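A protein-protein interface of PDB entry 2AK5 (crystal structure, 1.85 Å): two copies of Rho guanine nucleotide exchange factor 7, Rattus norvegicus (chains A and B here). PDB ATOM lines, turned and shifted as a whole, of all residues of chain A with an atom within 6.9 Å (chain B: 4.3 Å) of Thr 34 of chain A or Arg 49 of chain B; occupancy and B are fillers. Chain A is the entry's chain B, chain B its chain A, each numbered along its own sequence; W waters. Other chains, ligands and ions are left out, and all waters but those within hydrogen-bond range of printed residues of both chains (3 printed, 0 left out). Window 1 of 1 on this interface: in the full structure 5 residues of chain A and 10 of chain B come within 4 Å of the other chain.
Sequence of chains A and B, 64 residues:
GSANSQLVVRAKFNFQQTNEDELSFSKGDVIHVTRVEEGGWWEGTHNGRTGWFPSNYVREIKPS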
ATOM      1  N   ALA A   3       8.982  26.866  18.582  1.00  0.00           N
ATOM      2  CA  ALA A   3       7.873  27.792  18.799  1.00  0.00           C
ATOM      3  C   ALA A   3       6.557  27.160  19.236  1.00  0.00           C
ATOM      4  O   ALA A   3       6.160  26.095  18.749  1.00  0.00           O
ATOM      5  CB  ALA A   3       7.650  28.635  17.539  1.00  0.00           C
ATOM      6  N   ASN A   4       5.872  27.840  20.149  1.00  0.00           N
ATOM      7  CA  ASN A   4       4.560  27.409  20.607  1.00  0.00           C
ATOM      8  C   ASN A   4       4.575  25.999  21.184  1.00  0.00           C
ATOM      9  O   ASN A   4       3.636  25.230  20.987  1.00  0.00           O
ATOM     10  CB  ASN A   4       3.551  27.515  19.466  1.00  0.00           C
ATOM     11  CG  ASN A   4       3.593  28.869  18.781  1.00  0.00           C
ATOM     12  OD1 ASN A   4       3.817  28.967  17.569  1.00  0.00           O
ATOM     13  ND2 ASN A   4       3.401  29.926  19.560  1.00  0.00           N
ATOM     14  N   SER A   5       5.651  25.679  21.893  1.00  0.00           N
ATOM     15  CA  SER A   5       5.824  24.373  22.511  1.00  0.00           C
ATOM     16  C   SER A   5       4.979  24.279  23.771  1.00  0.00           C
ATOM     17  O   SER A   5       4.694  25.287  24.420  1.00  0.00           O
ATOM     18  CB  SER A   5       7.295  24.134  22.854  1.00  0.00           C
ATOM     19  OG  SER A   5       8.075  24.019  21.676  1.00  0.00           O
ATOM     20  N   GLN A   6       4.566  23.063  24.101  1.00  0.00           N
ATOM     21  CA  GLN A   6       3.769  22.847  25.295  1.00  0.00           C
ATOM     22  C   GLN A   6       4.601  23.210  26.515  1.00  0.00           C
ATOM     23  O   GLN A   6       5.780  22.859  26.602  1.00  0.00           O
ATOM     24  CB  GLN A   6       3.294  21.396  25.360  1.00  0.00           C
ATOM     25  CG  GLN A   6       2.215  21.137  26.408  1.00  0.00           C
ATOM     26  CD  GLN A   6       1.707  19.704  26.383  1.00  0.00           C
ATOM     27  OE1 GLN A   6       0.629  19.416  26.905  1.00  0.00           O
ATOM     28  NE2 GLN A   6       2.479  18.805  25.776  1.00  0.00           N
ATOM     29  N   LEU A   7       3.987  23.934  27.445  1.00  0.00           N
ATOM     30  CA  LEU A   7       4.662  24.366  28.661  1.00  0.00           C
ATOM     31  C   LEU A   7       4.974  23.208  29.602  1.00  0.00           C
ATOM     32  O   LEU A   7       4.178  22.285  29.756  1.00  0.00           O
ATOM     33  CB  LEU A   7       3.795  25.378  29.420  1.00  0.00           C
ATOM     34  CG  LEU A   7       3.678  26.819  28.919  1.00  0.00           C
ATOM     35  CD1 LEU A   7       3.109  26.892  27.509  1.00  0.00           C
ATOM     36  CD2 LEU A   7       2.805  27.615  29.881  1.00  0.00           C
ATOM     37  N   ILE A  31       4.759  18.559  35.437  1.00  0.00           N
ATOM     38  CA  ILE A  31       3.439  18.567  34.812  1.00  0.00           C
ATOM     39  C   ILE A  31       3.500  19.202  33.421  1.00  0.00           C
ATOM     40  O   ILE A  31       4.155  20.226  33.227  1.00  0.00           O
ATOM     41  CB  ILE A  31       2.433  19.347  35.690  1.00  0.00           C
ATOM     42  CG1 ILE A  31       2.430  18.819  37.128  1.00  0.00           C
ATOM     43  CG2 ILE A  31       1.026  19.304  35.085  1.00  0.00           C
ATOM     44  CD1 ILE A  31       1.668  19.704  38.095  1.00  0.00           C
ATOM     45  N   HIS A  32       2.831  18.574  32.458  1.00  0.00           N
ATOM     46  CA  HIS A  32       2.740  19.097  31.103  1.00  0.00           C
ATOM     47  C   HIS A  32       1.400  19.819  31.003  1.00  0.00           C
ATOM     48  O   HIS A  32       0.351  19.215  31.179  1.00  0.00           O
ATOM     49  CB  HIS A  32       2.833  17.965  30.080  1.00  0.00           C
ATOM     50  CG  HIS A  32       4.142  17.238  30.115  1.00  0.00           C
ATOM     51  ND1 HIS A  32       5.156  17.489  29.216  1.00  0.00           N
ATOM     52  CD2 HIS A  32       4.609  16.283  30.954  1.00  0.00           C
ATOM     53  CE1 HIS A  32       6.189  16.712  29.493  1.00  0.00           C
ATOM     54  NE2 HIS A  32       5.883  15.969  30.542  1.00  0.00           N
ATOM     55  N   VAL A  33       1.452  21.119  30.742  1.00  0.00           N
ATOM     56  CA  VAL A  33       0.261  21.967  30.728  1.00  0.00           C
ATOM     57  C   VAL A  33      -0.623  21.812  29.488  1.00  0.00           C
ATOM     58  O   VAL A  33      -0.135  21.886  28.362  1.00  0.00           O
ATOM     59  CB  VAL A  33       0.657  23.451  30.877  1.00  0.00           C
ATOM     60  CG1 VAL A  33      -0.581  24.342  30.919  1.00  0.00           C
ATOM     61  CG2 VAL A  33       1.525  23.659  32.121  1.00  0.00           C
ATOM     62  N   THR A  34      -1.926  21.619  29.705  1.00  0.00           N
ATOM     63  CA  THR A  34      -2.886  21.508  28.606  1.00  0.00           C
ATOM     64  C   THR A  34      -3.742  22.762  28.477  1.00  0.00           C
ATOM     65  O   THR A  34      -4.153  23.133  27.378  1.00  0.00           O
ATOM     66  CB  THR A  34      -3.793  20.288  28.793  1.00  0.00           C
ATOM     67  OG1 THR A  34      -4.340  20.300  30.117  1.00  0.00           O
ATOM     68  CG2 THR A  34      -2.976  19.005  28.745  1.00  0.00           C
ATOM     69  N   ARG A  35      -4.030  23.405  29.606  1.00  0.00           N
ATOM     70  CA  ARG A  35      -4.807  24.639  29.593  1.00  0.00           C
ATOM     71  C   ARG A  35      -4.220  25.687  30.528  1.00  0.00           C
ATOM     72  O   ARG A  35      -4.078  25.452  31.730  1.00  0.00           O
ATOM     73  CB  ARG A  35      -6.268  24.399  29.999  1.00  0.00           C
ATOM     74  CG  ARG A  35      -7.128  23.628  29.020  1.00  0.00           C
ATOM     75  CD  ARG A  35      -8.527  23.334  29.568  1.00  0.00           C
ATOM     76  NE  ARG A  35      -9.359  22.570  28.643  1.00  0.00           N
ATOM     77  CZ  ARG A  35     -10.179  23.118  27.755  1.00  0.00           C
ATOM     78  NH1 ARG A  35     -10.909  22.345  26.963  1.00  0.00           N
ATOM     79  NH2 ARG A  35     -10.269  24.436  27.654  1.00  0.00           N
ATOM     80  N   VAL A  36      -3.865  26.835  29.964  1.00  0.00           N
ATOM     81  CA  VAL A  36      -3.451  27.981  30.757  1.00  0.00           C
ATOM     82  C   VAL A  36      -4.670  28.898  30.828  1.00  0.00           C
ATOM     83  O   VAL A  36      -5.265  29.233  29.802  1.00  0.00           O
ATOM     84  CB  VAL A  36      -2.260  28.734  30.119  1.00  0.00           C
ATOM     85  CG1 VAL A  36      -2.012  30.058  30.835  1.00  0.00           C
ATOM     86  CG2 VAL A  36      -1.006  27.868  30.142  1.00  0.00           C
ATOM     87  N   TRP A  42      -4.720  26.023  36.441  1.00  0.00           N
ATOM     88  CA  TRP A  42      -4.307  25.565  35.117  1.00  0.00           C
ATOM     89  C   TRP A  42      -4.617  24.081  35.002  1.00  0.00           C
ATOM     90  O   TRP A  42      -4.788  23.401  36.014  1.00  0.00           O
ATOM     91  CB  TRP A  42      -2.803  25.745  34.930  1.00  0.00           C
ATOM     92  CG  TRP A  42      -2.341  27.166  34.719  1.00  0.00           C
ATOM     93  CD1 TRP A  42      -3.102  28.296  34.759  1.00  0.00           C
ATOM     94  CD2 TRP A  42      -1.006  27.594  34.430  1.00  0.00           C
ATOM     95  NE1 TRP A  42      -2.321  29.402  34.529  1.00  0.00           N
ATOM     96  CE2 TRP A  42      -1.029  28.998  34.314  1.00  0.00           C
ATOM     97  CE3 TRP A  42       0.217  26.930  34.258  1.00  0.00           C
ATOM     98  CZ2 TRP A  42       0.111  29.746  34.030  1.00  0.00           C
ATOM     99  CZ3 TRP A  42       1.347  27.671  33.978  1.00  0.00           C
ATOM    100  CH2 TRP A  42       1.290  29.069  33.868  1.00  0.00           C
ATOM    101  N   GLU A  43      -4.673  23.574  33.775  1.00  0.00           N
ATOM    102  CA  GLU A  43      -4.901  22.153  33.551  1.00  0.00           C
ATOM    103  C   GLU A  43      -3.618  21.547  32.990  1.00  0.00           C
ATOM    104  O   GLU A  43      -2.912  22.185  32.206  1.00  0.00           O
ATOM    105  CB  GLU A  43      -6.078  21.925  32.592  1.00  0.00           C
ATOM    106  CG  GLU A  43      -6.592  20.493  32.558  1.00  0.00           C
ATOM    107  CD  GLU A  43      -7.439  20.210  31.330  1.00  0.00           C
ATOM    108  OE1 GLU A  43      -6.931  20.398  30.203  1.00  0.00           O
ATOM    109  OE2 GLU A  43      -8.610  19.804  31.490  1.00  0.00           O
ATOM    110  N   GLY A  44      -3.300  20.328  33.412  1.00  0.00           N
ATOM    111  CA  GLY A  44      -2.112  19.649  32.936  1.00  0.00           C
ATOM    112  C   GLY A  44      -2.183  18.140  33.085  1.00  0.00           C
ATOM    113  O   GLY A  44      -3.146  17.607  33.630  1.00  0.00           O
ATOM    114  N   THR A  45      -1.169  17.447  32.583  1.00  0.00           N
ATOM    115  CA  THR A  45      -1.121  15.999  32.727  1.00  0.00           C
ATOM    116  C   THR A  45       0.051  15.592  33.602  1.00  0.00           C
ATOM    117  O   THR A  45       1.105  16.228  33.598  1.00  0.00           O
ATOM    118  CB  THR A  45      -1.014  15.288  31.370  1.00  0.00           C
ATOM    119  OG1 THR A  45       0.209  15.664  30.727  1.00  0.00           O
ATOM    120  CG2 THR A  45      -2.088  15.774  30.428  1.00  0.00           C
ATOM    121  N   THR A  50      -5.169  13.697  33.533  1.00  0.00           N
ATOM    122  CA  THR A  50      -5.326  15.114  33.245  1.00  0.00           C
ATOM    123  C   THR A  50      -6.202  15.752  34.307  1.00  0.00           C
ATOM    124  O   THR A  50      -7.292  15.259  34.608  1.00  0.00           O
ATOM    125  CB  THR A  50      -5.985  15.286  31.868  1.00  0.00           C
ATOM    126  OG1 THR A  50      -5.138  14.720  30.862  1.00  0.00           O
ATOM    127  CG2 THR A  50      -6.080  16.762  31.488  1.00  0.00           C
ATOM    128  N   GLY A  51      -5.729  16.856  34.873  1.00  0.00           N
ATOM    129  CA  GLY A  51      -6.499  17.543  35.884  1.00  0.00           C
ATOM    130  C   GLY A  51      -6.071  18.969  36.143  1.00  0.00           C
ATOM    131  O   GLY A  51      -5.031  19.430  35.669  1.00  0.00           O
ATOM    132  N   PHE A  53      -5.008  22.263  38.559  1.00  0.00           N
ATOM    133  CA  PHE A  53      -4.089  22.487  39.667  1.00  0.00           C
ATOM    134  C   PHE A  53      -3.838  23.979  39.853  1.00  0.00           C
ATOM    135  O   PHE A  53      -4.031  24.774  38.925  1.00  0.00           O
ATOM    136  CB  PHE A  53      -2.773  21.730  39.446  1.00  0.00           C
ATOM    137  CG  PHE A  53      -1.995  22.192  38.240  1.00  0.00           C
ATOM    138  CD1 PHE A  53      -1.010  23.161  38.363  1.00  0.00           C
ATOM    139  CD2 PHE A  53      -2.247  21.651  36.983  1.00  0.00           C
ATOM    140  CE1 PHE A  53      -0.294  23.592  37.258  1.00  0.00           C
ATOM    141  CE2 PHE A  53      -1.541  22.081  35.872  1.00  0.00           C
ATOM    142  CZ  PHE A  53      -0.557  23.049  36.007  1.00  0.00           C
ATOM    143  N   LEU B  23      -4.554  30.422  22.271  1.00  0.00           N
ATOM    144  CA  LEU B  23      -3.685  29.431  21.650  1.00  0.00           C
ATOM    145  C   LEU B  23      -2.863  30.046  20.519  1.00  0.00           C
ATOM    146  O   LEU B  23      -3.349  30.167  19.400  1.00  0.00           O
ATOM    147  CB  LEU B  23      -4.536  28.297  21.071  1.00  0.00           C
ATOM    148  CG  LEU B  23      -3.781  27.158  20.383  1.00  0.00           C
ATOM    149  CD1 LEU B  23      -3.024  26.359  21.424  1.00  0.00           C
ATOM    150  CD2 LEU B  23      -4.718  26.263  19.575  1.00  0.00           C
ATOM    151  N   SER B  24      -1.627  30.428  20.816  1.00  0.00           N
ATOM    152  CA  SER B  24      -0.744  30.978  19.796  1.00  0.00           C
ATOM    153  C   SER B  24      -0.336  29.871  18.836  1.00  0.00           C
ATOM    154  O   SER B  24      -0.169  28.723  19.236  1.00  0.00           O
ATOM    155  CB  SER B  24       0.509  31.574  20.431  1.00  0.00           C
ATOM    156  OG  SER B  24       0.193  32.665  21.276  1.00  0.00           O
ATOM    157  N   GLY B  44      -9.413  25.237  20.361  1.00  0.00           N
ATOM    158  CA  GLY B  44      -8.731  24.144  19.692  1.00  0.00           C
ATOM    159  C   GLY B  44      -7.490  23.651  20.397  1.00  0.00           C
ATOM    160  O   GLY B  44      -7.043  24.236  21.382  1.00  0.00           O
ATOM    161  N   THR B  45      -6.917  22.577  19.864  1.00  0.00           N
ATOM    162  CA  THR B  45      -5.733  21.968  20.439  1.00  0.00           C
ATOM    163  C   THR B  45      -4.603  21.837  19.433  1.00  0.00           C
ATOM    164  O   THR B  45      -4.787  21.293  18.346  1.00  0.00           O
ATOM    165  CB  THR B  45      -6.057  20.568  20.971  1.00  0.00           C
ATOM    166  OG1 THR B  45      -7.181  20.629  21.859  1.00  0.00           O
ATOM    167  CG2 THR B  45      -4.903  20.045  21.841  1.00  0.00           C
ATOM    168  N   HIS B  46      -3.437  22.339  19.816  1.00  0.00           N
ATOM    169  CA  HIS B  46      -2.217  22.191  19.035  1.00  0.00           C
ATOM    170  C   HIS B  46      -1.071  21.992  20.014  1.00  0.00           C
ATOM    171  O   HIS B  46      -0.946  22.742  20.977  1.00  0.00           O
ATOM    172  CB  HIS B  46      -1.949  23.416  18.159  1.00  0.00           C
ATOM    173  CG  HIS B  46      -0.595  23.401  17.519  1.00  0.00           C
ATOM    174  ND1 HIS B  46      -0.362  22.828  16.284  1.00  0.00           N
ATOM    175  CD2 HIS B  46       0.598  23.870  17.948  1.00  0.00           C
ATOM    176  CE1 HIS B  46       0.916  22.955  15.980  1.00  0.00           C
ATOM    177  NE2 HIS B  46       1.519  23.591  16.967  1.00  0.00           N
ATOM    178  N   ASN B  47      -0.233  20.989  19.763  1.00  0.00           N
ATOM    179  CA  ASN B  47       0.860  20.648  20.668  1.00  0.00           C
ATOM    180  C   ASN B  47       0.348  20.287  22.065  1.00  0.00           C
ATOM    181  O   ASN B  47       1.008  20.556  23.059  1.00  0.00           O
ATOM    182  CB  ASN B  47       1.897  21.781  20.758  1.00  0.00           C
ATOM    183  CG  ASN B  47       2.926  21.727  19.642  1.00  0.00           C
ATOM    184  OD1 ASN B  47       3.644  22.709  19.380  1.00  0.00           O
ATOM    185  ND2 ASN B  47       3.018  20.586  18.988  1.00  0.00           N
ATOM    186  N   GLY B  48      -0.844  19.702  22.132  1.00  0.00           N
ATOM    187  CA  GLY B  48      -1.413  19.291  23.407  1.00  0.00           C
ATOM    188  C   GLY B  48      -1.936  20.427  24.262  1.00  0.00           C
ATOM    189  O   GLY B  48      -2.397  20.215  25.385  1.00  0.00           O
ATOM    190  N   ARG B  49      -1.848  21.645  23.751  1.00  0.00           N
ATOM    191  CA  ARG B  49      -2.373  22.770  24.497  1.00  0.00           C
ATOM    192  C   ARG B  49      -3.702  23.211  23.885  1.00  0.00           C
ATOM    193  O   ARG B  49      -3.866  23.269  22.659  1.00  0.00           O
ATOM    194  CB  ARG B  49      -1.333  23.891  24.648  1.00  0.00           C
ATOM    195  CG  ARG B  49      -1.103  24.706  23.440  1.00  0.00           C
ATOM    196  CD  ARG B  49       0.362  24.933  23.076  1.00  0.00           C
ATOM    197  NE  ARG B  49       0.402  25.052  21.633  1.00  0.00           N
ATOM    198  CZ  ARG B  49       0.415  26.191  20.972  1.00  0.00           C
ATOM    199  NH1 ARG B  49       0.442  27.348  21.618  1.00  0.00           N
ATOM    200  NH2 ARG B  49       0.404  26.172  19.651  1.00  0.00           N
ATOM    201  N   THR B  50      -4.669  23.466  24.754  1.00  0.00           N
ATOM    202  CA  THR B  50      -6.006  23.834  24.316  1.00  0.00           C
ATOM    203  C   THR B  50      -6.294  25.273  24.710  1.00  0.00           C
ATOM    204  O   THR B  50      -6.069  25.673  25.850  1.00  0.00           O
ATOM    205  CB  THR B  50      -7.038  22.868  24.919  1.00  0.00           C
ATOM    206  OG1 THR B  50      -6.814  21.553  24.386  1.00  0.00           O
ATOM    207  CG2 THR B  50      -8.440  23.212  24.433  1.00  0.00           C
ATOM    208  N   GLY B  51      -6.755  26.061  23.749  1.00  0.00           N
ATOM    209  CA  GLY B  51      -7.020  27.459  24.005  1.00  0.00           C
ATOM    210  C   GLY B  51      -7.820  28.095  22.891  1.00  0.00           C
ATOM    211  O   GLY B  51      -8.222  27.432  21.928  1.00  0.00           O
HETATM  212  O   HOH W   1       6.190  23.492  18.457  1.00  0.00           O
HETATM  213  O   HOH W   2      -6.673  27.655  27.916  1.00  0.00           O
HETATM  214  O   HOH W   3      -3.558  26.803  27.008  1.00  0.00           O
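O of His 46 of chain B lies within hydrogen-bond range of NE of Arg 49 of chain B (2.8 Å). The side-chain hydroxyl (OG1) of Thr 45 of chain B is in hydrogen-bond range of the side-chain hydroxyl (OG1) of Thr 50 of chain B, at 2.7 Å. OE1 of Glu 43 of chain A lies within salt-bridge range of NE of Arg 35 of chain A (3.6 Å). O of Val 33 of chain A sits close to OE1 of Gln 6 of chain A (3.0 Å). The backbone carbonyl oxygen of Ser 24 of chain B is in hydrogen-bond range of the guanidinium group of Arg 49 of chain B (2.6 Å). The side-chain hydroxyl of Thr 34 of chain A is in hydrogen-bond range of the side-chain carboxylate of Glu 43 of chain A (2.6 Å).
Of the printed residues of chain B, Asn 4 of chain A touches Ser 24, Asn 47 and Arg 49. Of the printed residues of chain B, Gln 6 of chain A touches Asn 47 and Gly 48. Of the printed residues of chain B, Arg 35 of chain A touches Thr 50. Thr 50 of chain A touches none of the printed residues of chain B. Of the printed residues of chain A, Asn 47 of chain B touches Asn 4 and Gln 6. Of chain A, only Asn 4 (3.3 Å) and Thr 34 (3.4 Å) come within 4 Å of Arg 49 of chain B. Of the printed residues of chain A, Thr 50 of chain B touches Thr 34 and Arg 35. The nearest printed residue of chain B that does not touch Thr 34 of chain A is Gly 51 of chain B (5.3 Å). The nearest residue of chain A that does not touch Arg 49 of chain B is Val 33 of chain A (4.4 Å).
O of Asn 4 of chain A is in hydrogen-bond range of NE of Arg 49 of chain B (3.3 Å). The side-chain amide oxygen (OD1) of Asn 47 of chain B lies close to the backbone carbonyl oxygen (O) of Asn 4 of chain A (3.0 Å). O of Thr 34 of chain A sits at hydrogen-bond distance from N of Thr 50 of chain B (2.7 Å). The side-chain amide oxygen of Gln 6 of chain A lies close to the backbone carbonyl oxygen of Gly 48 of chain B (3.5 Å).
Printed residues of chain B that touch a printed residue of chain A: Ser 24, Asn 47, Gly 48, Arg 49 and Thr 50. Printed residues of chain A that touch a printed residue of chain B: Asn 4, Gln 6, Thr 34 and Arg 35. Among the printed residues, no Asp or Glu carboxylate lies within 4 Å of a Lys or Arg side-chain nitrogen of the other chain.
Water W1 lies within hydrogen-bond range of O of Ala 3 of chain A (2.6 Å) and OD1 of Asn 47 of chain B (2.8 Å). Water W2 lies within hydrogen-bond range of the backbone carbonyl oxygen (O) of Val 36 of chain A and the backbone carbonyl oxygen (O) of Thr 50 of chain B. Water W3 lies within hydrogen-bond range of N of Val 36 of chain A (3.0 Å) and O of Thr 50 of chain B (3.0 Å).
Positions printed for both chains: 44, 45, 50 and 51.
Among the printed residues, merely in contact across the chains: Gln 6 of chain A with Asn 47 of chain B (3.4 Å), Thr 34 of chain A with Arg 49 of chain B (3.4 Å), Asn 4 of chain A with Ser 24 of chain B (3.4 Å), Thr 34 of chain A with Gly 48 of chain B (3.5 Å) and Arg 35 of chain A with Thr 50 of chain B (3.6 Å).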
